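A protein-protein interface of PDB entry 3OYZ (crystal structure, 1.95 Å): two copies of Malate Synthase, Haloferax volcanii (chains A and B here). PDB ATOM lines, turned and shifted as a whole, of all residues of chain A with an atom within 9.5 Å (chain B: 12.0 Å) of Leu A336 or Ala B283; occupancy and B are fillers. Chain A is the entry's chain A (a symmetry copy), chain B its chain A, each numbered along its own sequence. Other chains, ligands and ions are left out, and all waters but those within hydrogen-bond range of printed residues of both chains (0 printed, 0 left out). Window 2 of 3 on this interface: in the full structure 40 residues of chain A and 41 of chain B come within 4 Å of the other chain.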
ATOM      1  N   THR A 203     -29.859  28.445 -36.602  1.00  0.00           N
ATOM      2  CA  THR A 203     -30.903  28.636 -35.585  1.00  0.00           C
ATOM      3  C   THR A 203     -32.225  29.294 -36.053  1.00  0.00           C
ATOM      4  O   THR A 203     -33.244  29.184 -35.377  1.00  0.00           O
ATOM      5  CB  THR A 203     -30.315  29.391 -34.354  1.00  0.00           C
ATOM      6  OG1 THR A 203     -30.053  30.769 -34.686  1.00  0.00           O
ATOM      7  CG2 THR A 203     -28.974  28.780 -33.911  1.00  0.00           C
ATOM      8  N   ASP A 237     -33.650  38.986 -23.893  1.00  0.00           N
ATOM      9  CA  ASP A 237     -32.184  38.992 -23.846  1.00  0.00           C
ATOM     10  C   ASP A 237     -31.716  40.430 -23.626  1.00  0.00           C
ATOM     11  O   ASP A 237     -31.403  41.184 -24.568  1.00  0.00           O
ATOM     12  CB  ASP A 237     -31.651  38.337 -25.137  1.00  0.00           C
ATOM     13  CG  ASP A 237     -30.144  38.197 -25.173  1.00  0.00           C
ATOM     14  OD1 ASP A 237     -29.440  38.505 -24.189  1.00  0.00           O
ATOM     15  OD2 ASP A 237     -29.651  37.745 -26.227  1.00  0.00           O
ATOM     16  N   LEU A 329     -29.357  31.941 -13.097  1.00  0.00           N
ATOM     17  CA  LEU A 329     -28.448  31.058 -13.839  1.00  0.00           C
ATOM     18  C   LEU A 329     -29.087  30.749 -15.198  1.00  0.00           C
ATOM     19  O   LEU A 329     -28.403  30.647 -16.224  1.00  0.00           O
ATOM     20  CB  LEU A 329     -28.159  29.752 -13.085  1.00  0.00           C
ATOM     21  CG  LEU A 329     -27.645  28.567 -13.918  1.00  0.00           C
ATOM     22  CD1 LEU A 329     -26.116  28.428 -13.867  1.00  0.00           C
ATOM     23  CD2 LEU A 329     -28.360  27.251 -13.574  1.00  0.00           C
ATOM     24  N   ARG A 330     -30.410  30.588 -15.166  1.00  0.00           N
ATOM     25  CA  ARG A 330     -31.243  30.488 -16.357  1.00  0.00           C
ATOM     26  C   ARG A 330     -30.830  31.526 -17.404  1.00  0.00           C
ATOM     27  O   ARG A 330     -30.580  31.156 -18.546  1.00  0.00           O
ATOM     28  CB  ARG A 330     -32.711  30.653 -15.972  1.00  0.00           C
ATOM     29  CG  ARG A 330     -33.685  30.054 -16.967  1.00  0.00           C
ATOM     30  CD  ARG A 330     -35.115  30.160 -16.460  1.00  0.00           C
ATOM     31  NE  ARG A 330     -35.184  29.909 -15.021  1.00  0.00           N
ATOM     32  CZ  ARG A 330     -35.155  28.699 -14.469  1.00  0.00           C
ATOM     33  NH1 ARG A 330     -35.076  27.622 -15.242  1.00  0.00           N
ATOM     34  NH2 ARG A 330     -35.215  28.584 -13.147  1.00  0.00           N
ATOM     35  N   GLU A 331     -30.723  32.800 -17.024  1.00  0.00           N
ATOM     36  CA  GLU A 331     -30.302  33.846 -17.967  1.00  0.00           C
ATOM     37  C   GLU A 331     -28.909  33.687 -18.595  1.00  0.00           C
ATOM     38  O   GLU A 331     -28.800  33.813 -19.816  1.00  0.00           O
ATOM     39  CB  GLU A 331     -30.609  35.289 -17.512  1.00  0.00           C
ATOM     40  CG  GLU A 331     -31.915  35.863 -18.119  1.00  0.00           C
ATOM     41  CD  GLU A 331     -31.865  37.347 -18.540  1.00  0.00           C
ATOM     42  OE1 GLU A 331     -31.856  38.231 -17.653  1.00  0.00           O
ATOM     43  OE2 GLU A 331     -31.872  37.658 -19.758  1.00  0.00           O
ATOM     44  N   GLU A 332     -27.856  33.350 -17.854  1.00  0.00           N
ATOM     45  CA  GLU A 332     -26.615  33.056 -18.583  1.00  0.00           C
ATOM     46  C   GLU A 332     -26.639  31.694 -19.301  1.00  0.00           C
ATOM     47  O   GLU A 332     -25.860  31.464 -20.233  1.00  0.00           O
ATOM     48  CB  GLU A 332     -25.330  33.342 -17.788  1.00  0.00           C
ATOM     49  CG  GLU A 332     -24.128  33.754 -18.676  1.00  0.00           C
ATOM     50  CD  GLU A 332     -23.405  35.047 -18.263  1.00  0.00           C
ATOM     51  OE1 GLU A 332     -22.260  35.282 -18.715  1.00  0.00           O
ATOM     52  OE2 GLU A 332     -23.969  35.858 -17.498  1.00  0.00           O
ATOM     53  N   LEU A 333     -27.575  30.822 -18.925  1.00  0.00           N
ATOM     54  CA  LEU A 333     -27.811  29.569 -19.662  1.00  0.00           C
ATOM     55  C   LEU A 333     -28.451  29.727 -21.052  1.00  0.00           C
ATOM     56  O   LEU A 333     -28.007  29.094 -22.012  1.00  0.00           O
ATOM     57  CB  LEU A 333     -28.605  28.564 -18.820  1.00  0.00           C
ATOM     58  CG  LEU A 333     -27.871  27.419 -18.108  1.00  0.00           C
ATOM     59  CD1 LEU A 333     -28.776  26.188 -18.132  1.00  0.00           C
ATOM     60  CD2 LEU A 333     -26.531  27.054 -18.749  1.00  0.00           C
ATOM     61  N   LEU A 334     -29.500  30.544 -21.141  1.00  0.00           N
ATOM     62  CA  LEU A 334     -30.104  30.948 -22.411  1.00  0.00           C
ATOM     63  C   LEU A 334     -29.097  31.719 -23.254  1.00  0.00           C
ATOM     64  O   LEU A 334     -29.014  31.518 -24.461  1.00  0.00           O
ATOM     65  CB  LEU A 334     -31.337  31.813 -22.178  1.00  0.00           C
ATOM     66  CG  LEU A 334     -32.508  31.069 -21.538  1.00  0.00           C
ATOM     67  CD1 LEU A 334     -33.522  32.033 -20.924  1.00  0.00           C
ATOM     68  CD2 LEU A 334     -33.139  30.112 -22.526  1.00  0.00           C
ATOM     69  N   GLY A 335     -28.337  32.607 -22.625  1.00  0.00           N
ATOM     70  CA  GLY A 335     -27.173  33.207 -23.259  1.00  0.00           C
ATOM     71  C   GLY A 335     -26.236  32.171 -23.863  1.00  0.00           C
ATOM     72  O   GLY A 335     -25.524  32.487 -24.812  1.00  0.00           O
ATOM     73  N   LEU A 336     -26.232  30.936 -23.356  1.00  0.00           N
ATOM     74  CA  LEU A 336     -25.285  29.926 -23.853  1.00  0.00           C
ATOM     75  C   LEU A 336     -25.853  28.813 -24.751  1.00  0.00           C
ATOM     76  O   LEU A 336     -25.118  28.177 -25.513  1.00  0.00           O
ATOM     77  CB  LEU A 336     -24.451  29.325 -22.709  1.00  0.00           C
ATOM     78  CG  LEU A 336     -23.564  30.220 -21.832  1.00  0.00           C
ATOM     79  CD1 LEU A 336     -23.133  29.425 -20.602  1.00  0.00           C
ATOM     80  CD2 LEU A 336     -22.362  30.810 -22.603  1.00  0.00           C
ATOM     81  N   THR A 337     -27.157  28.571 -24.661  1.00  0.00           N
ATOM     82  CA  THR A 337     -27.789  27.580 -25.512  1.00  0.00           C
ATOM     83  C   THR A 337     -28.334  28.174 -26.818  1.00  0.00           C
ATOM     84  O   THR A 337     -28.658  29.358 -26.881  1.00  0.00           O
ATOM     85  CB  THR A 337     -28.937  26.900 -24.776  1.00  0.00           C
ATOM     86  OG1 THR A 337     -29.885  27.901 -24.382  1.00  0.00           O
ATOM     87  CG2 THR A 337     -28.393  26.219 -23.541  1.00  0.00           C
ATOM     88  N   SER A 338     -28.428  27.355 -27.859  1.00  0.00           N
ATOM     89  CA  SER A 338     -29.291  27.650 -29.000  1.00  0.00           C
ATOM     90  C   SER A 338     -29.904  26.362 -29.520  1.00  0.00           C
ATOM     91  O   SER A 338     -29.361  25.281 -29.300  1.00  0.00           O
ATOM     92  CB  SER A 338     -28.516  28.347 -30.121  1.00  0.00           C
ATOM     93  OG  SER A 338     -27.222  27.801 -30.251  1.00  0.00           O
ATOM     94  N   TYR A 339     -31.045  26.475 -30.187  1.00  0.00           N
ATOM     95  CA  TYR A 339     -31.648  25.356 -30.849  1.00  0.00           C
ATOM     96  C   TYR A 339     -31.439  25.459 -32.364  1.00  0.00           C
ATOM     97  O   TYR A 339     -31.446  26.565 -32.931  1.00  0.00           O
ATOM     98  CB  TYR A 339     -33.134  25.417 -30.553  1.00  0.00           C
ATOM     99  CG  TYR A 339     -33.842  24.219 -31.056  1.00  0.00           C
ATOM    100  CD1 TYR A 339     -33.440  22.945 -30.638  1.00  0.00           C
ATOM    101  CD2 TYR A 339     -34.926  24.331 -31.913  1.00  0.00           C
ATOM    102  CE1 TYR A 339     -34.090  21.804 -31.052  1.00  0.00           C
ATOM    103  CE2 TYR A 339     -35.578  23.199 -32.351  1.00  0.00           C
ATOM    104  CZ  TYR A 339     -35.152  21.947 -31.901  1.00  0.00           C
ATOM    105  OH  TYR A 339     -35.754  20.784 -32.296  1.00  0.00           O
ATOM    106  N   ILE A 381     -35.045  25.569 -19.140  1.00  0.00           N
ATOM    107  CA  ILE A 381     -35.015  26.914 -19.733  1.00  0.00           C
ATOM    108  C   ILE A 381     -36.130  27.173 -20.759  1.00  0.00           C
ATOM    109  O   ILE A 381     -36.747  26.233 -21.280  1.00  0.00           O
ATOM    110  CB  ILE A 381     -33.652  27.227 -20.401  1.00  0.00           C
ATOM    111  CG1 ILE A 381     -33.298  26.136 -21.421  1.00  0.00           C
ATOM    112  CG2 ILE A 381     -32.554  27.457 -19.367  1.00  0.00           C
ATOM    113  CD1 ILE A 381     -32.201  26.524 -22.399  1.00  0.00           C
ATOM    114  N   LYS A 383     -36.753  29.926 -24.056  1.00  0.00           N
ATOM    115  CA  LYS A 383     -36.208  30.940 -24.975  1.00  0.00           C
ATOM    116  C   LYS A 383     -37.382  31.612 -25.682  1.00  0.00           C
ATOM    117  O   LYS A 383     -38.186  30.901 -26.281  1.00  0.00           O
ATOM    118  CB  LYS A 383     -35.313  30.248 -26.002  1.00  0.00           C
ATOM    119  CG  LYS A 383     -34.003  30.955 -26.289  1.00  0.00           C
ATOM    120  CD  LYS A 383     -33.125  30.050 -27.151  1.00  0.00           C
ATOM    121  CE  LYS A 383     -31.675  30.485 -27.061  1.00  0.00           C
ATOM    122  NZ  LYS A 383     -31.116  30.113 -25.741  1.00  0.00           N
ATOM    123  N   SER B 278     -31.916  19.965 -32.425  1.00  0.00           N
ATOM    124  CA  SER B 278     -30.554  19.722 -31.989  1.00  0.00           C
ATOM    125  C   SER B 278     -30.229  20.950 -31.131  1.00  0.00           C
ATOM    126  O   SER B 278     -30.401  22.084 -31.591  1.00  0.00           O
ATOM    127  CB  SER B 278     -29.690  19.545 -33.233  1.00  0.00           C
ATOM    128  OG  SER B 278     -28.328  19.727 -32.952  1.00  0.00           O
ATOM    129  N   TRP B 279     -29.902  20.744 -29.855  1.00  0.00           N
ATOM    130  CA  TRP B 279     -29.566  21.829 -28.934  1.00  0.00           C
ATOM    131  C   TRP B 279     -28.053  21.994 -28.850  1.00  0.00           C
ATOM    132  O   TRP B 279     -27.339  21.003 -28.871  1.00  0.00           O
ATOM    133  CB  TRP B 279     -30.166  21.584 -27.546  1.00  0.00           C
ATOM    134  CG  TRP B 279     -31.639  21.930 -27.410  1.00  0.00           C
ATOM    135  CD1 TRP B 279     -32.698  21.113 -27.696  1.00  0.00           C
ATOM    136  CD2 TRP B 279     -32.204  23.191 -26.980  1.00  0.00           C
ATOM    137  NE1 TRP B 279     -33.889  21.774 -27.434  1.00  0.00           N
ATOM    138  CE2 TRP B 279     -33.611  23.047 -26.997  1.00  0.00           C
ATOM    139  CE3 TRP B 279     -31.657  24.414 -26.555  1.00  0.00           C
ATOM    140  CZ2 TRP B 279     -34.483  24.108 -26.660  1.00  0.00           C
ATOM    141  CZ3 TRP B 279     -32.504  25.440 -26.191  1.00  0.00           C
ATOM    142  CH2 TRP B 279     -33.912  25.282 -26.235  1.00  0.00           C
ATOM    143  N   LEU B 280     -27.530  23.214 -28.792  1.00  0.00           N
ATOM    144  CA  LEU B 280     -26.085  23.399 -28.688  1.00  0.00           C
ATOM    145  C   LEU B 280     -25.782  24.140 -27.399  1.00  0.00           C
ATOM    146  O   LEU B 280     -26.572  24.989 -26.972  1.00  0.00           O
ATOM    147  CB  LEU B 280     -25.486  24.129 -29.901  1.00  0.00           C
ATOM    148  CG  LEU B 280     -25.808  23.537 -31.277  1.00  0.00           C
ATOM    149  CD1 LEU B 280     -25.468  24.507 -32.413  1.00  0.00           C
ATOM    150  CD2 LEU B 280     -25.113  22.194 -31.502  1.00  0.00           C
ATOM    151  N   LEU B 281     -24.649  23.796 -26.788  1.00  0.00           N
ATOM    152  CA  LEU B 281     -24.176  24.474 -25.582  1.00  0.00           C
ATOM    153  C   LEU B 281     -22.848  25.136 -25.885  1.00  0.00           C
ATOM    154  O   LEU B 281     -21.910  24.469 -26.331  1.00  0.00           O
ATOM    155  CB  LEU B 281     -24.043  23.528 -24.382  1.00  0.00           C
ATOM    156  CG  LEU B 281     -23.851  24.228 -23.027  1.00  0.00           C
ATOM    157  CD1 LEU B 281     -25.078  25.009 -22.539  1.00  0.00           C
ATOM    158  CD2 LEU B 281     -23.386  23.248 -21.945  1.00  0.00           C
ATOM    159  N   ASP B 282     -22.803  26.445 -25.641  1.00  0.00           N
ATOM    160  CA  ASP B 282     -21.777  27.301 -26.238  1.00  0.00           C
ATOM    161  C   ASP B 282     -20.672  27.702 -25.263  1.00  0.00           C
ATOM    162  O   ASP B 282     -19.729  28.392 -25.674  1.00  0.00           O
ATOM    163  CB  ASP B 282     -22.365  28.537 -26.953  1.00  0.00           C
ATOM    164  CG  ASP B 282     -23.032  28.212 -28.314  1.00  0.00           C
ATOM    165  OD1 ASP B 282     -22.365  27.675 -29.242  1.00  0.00           O
ATOM    166  OD2 ASP B 282     -24.245  28.529 -28.447  1.00  0.00           O
ATOM    167  N   ALA B 283     -20.773  27.274 -24.003  1.00  0.00           N
ATOM    168  CA  ALA B 283     -19.658  27.495 -23.075  1.00  0.00           C
ATOM    169  C   ALA B 283     -18.503  26.532 -23.385  1.00  0.00           C
ATOM    170  O   ALA B 283     -18.698  25.316 -23.471  1.00  0.00           O
ATOM    171  CB  ALA B 283     -20.093  27.470 -21.606  1.00  0.00           C
ATOM    172  N   ASP B 284     -17.316  27.112 -23.574  1.00  0.00           N
ATOM    173  CA  ASP B 284     -16.213  26.521 -24.343  1.00  0.00           C
ATOM    174  C   ASP B 284     -16.607  25.505 -25.417  1.00  0.00           C
ATOM    175  O   ASP B 284     -16.700  25.858 -26.592  1.00  0.00           O
ATOM    176  CB  ASP B 284     -15.107  25.986 -23.428  1.00  0.00           C
ATOM    177  CG  ASP B 284     -14.161  27.086 -22.976  1.00  0.00           C
ATOM    178  OD1 ASP B 284     -12.945  26.978 -23.249  1.00  0.00           O
ATOM    179  OD2 ASP B 284     -14.630  28.080 -22.379  1.00  0.00           O
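N of Asp B282 is in hydrogen-bond range of O of Leu A336 (2.9 Å).
The backbone carbonyl oxygen of Ser A338 is in hydrogen-bond range of the backbone NH of Leu B280, 2.8 Å away.
The side-chain hydroxyl (OG1) of Thr A337 is in hydrogen-bond range of the backbone carbonyl oxygen (O) of Leu A333.
The backbone carbonyl oxygen of Thr A337 sits at hydrogen-bond distance from the side-chain amino group of Lys A383 (2.8 Å).
Among the printed residues, merely in contact across the chains: Leu A336 with Leu B280, Leu A336 with Leu B281, Leu A336 with Ala B283, Thr A337 with Leu B280, Thr A337 with Leu B281, Ser A338 with Trp B279, Ser A338 with Asp B282, Tyr A339 with Ser B278, Tyr A339 with Trp B279 and Ile A381 with Trp B279.
No residue of chain B comes within 4 Å of Glu A332.
No residue of chain B comes within 4 Å of Leu A333.
Gly A335 touches none of the printed residues of chain B.
Of chain B, only Leu B280, Leu B281, Asp B282 and Ala B283 come within 4 Å of Leu A336.
Of the printed residues of chain B, Tyr A339 touches Ser B278 (3.2 Å) and Trp B279 (3.4 Å).
Printed residues of chain A within 4 Å of Ser B278: Tyr A339.
Of the printed residues of chain A, Trp B279 touches Ser A338, Tyr A339 and Ile A381.
Printed residues of chain A within 4 Å of Leu B280: Leu A336 (3.8 Å), Thr A337 (3.2 Å) and Ser A338 (2.8 Å).
Asp B282 touches just these residues of chain A: Leu A336 and Ser A338.
Of chain A, only Leu A336 (3.8 Å) comes within 4 Å of Ala B283.
The nearest residue of chain A that does not touch Ala B283 is Thr A337 (6.5 Å).
Of the 7 printed residues of chain B, 6 touch a printed residue of chain A.
Among the printed residues, no Asp or Glu carboxylate lies within 4 Å of a Lys or Arg side-chain nitrogen of the other chain.
No position is printed for both chains.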
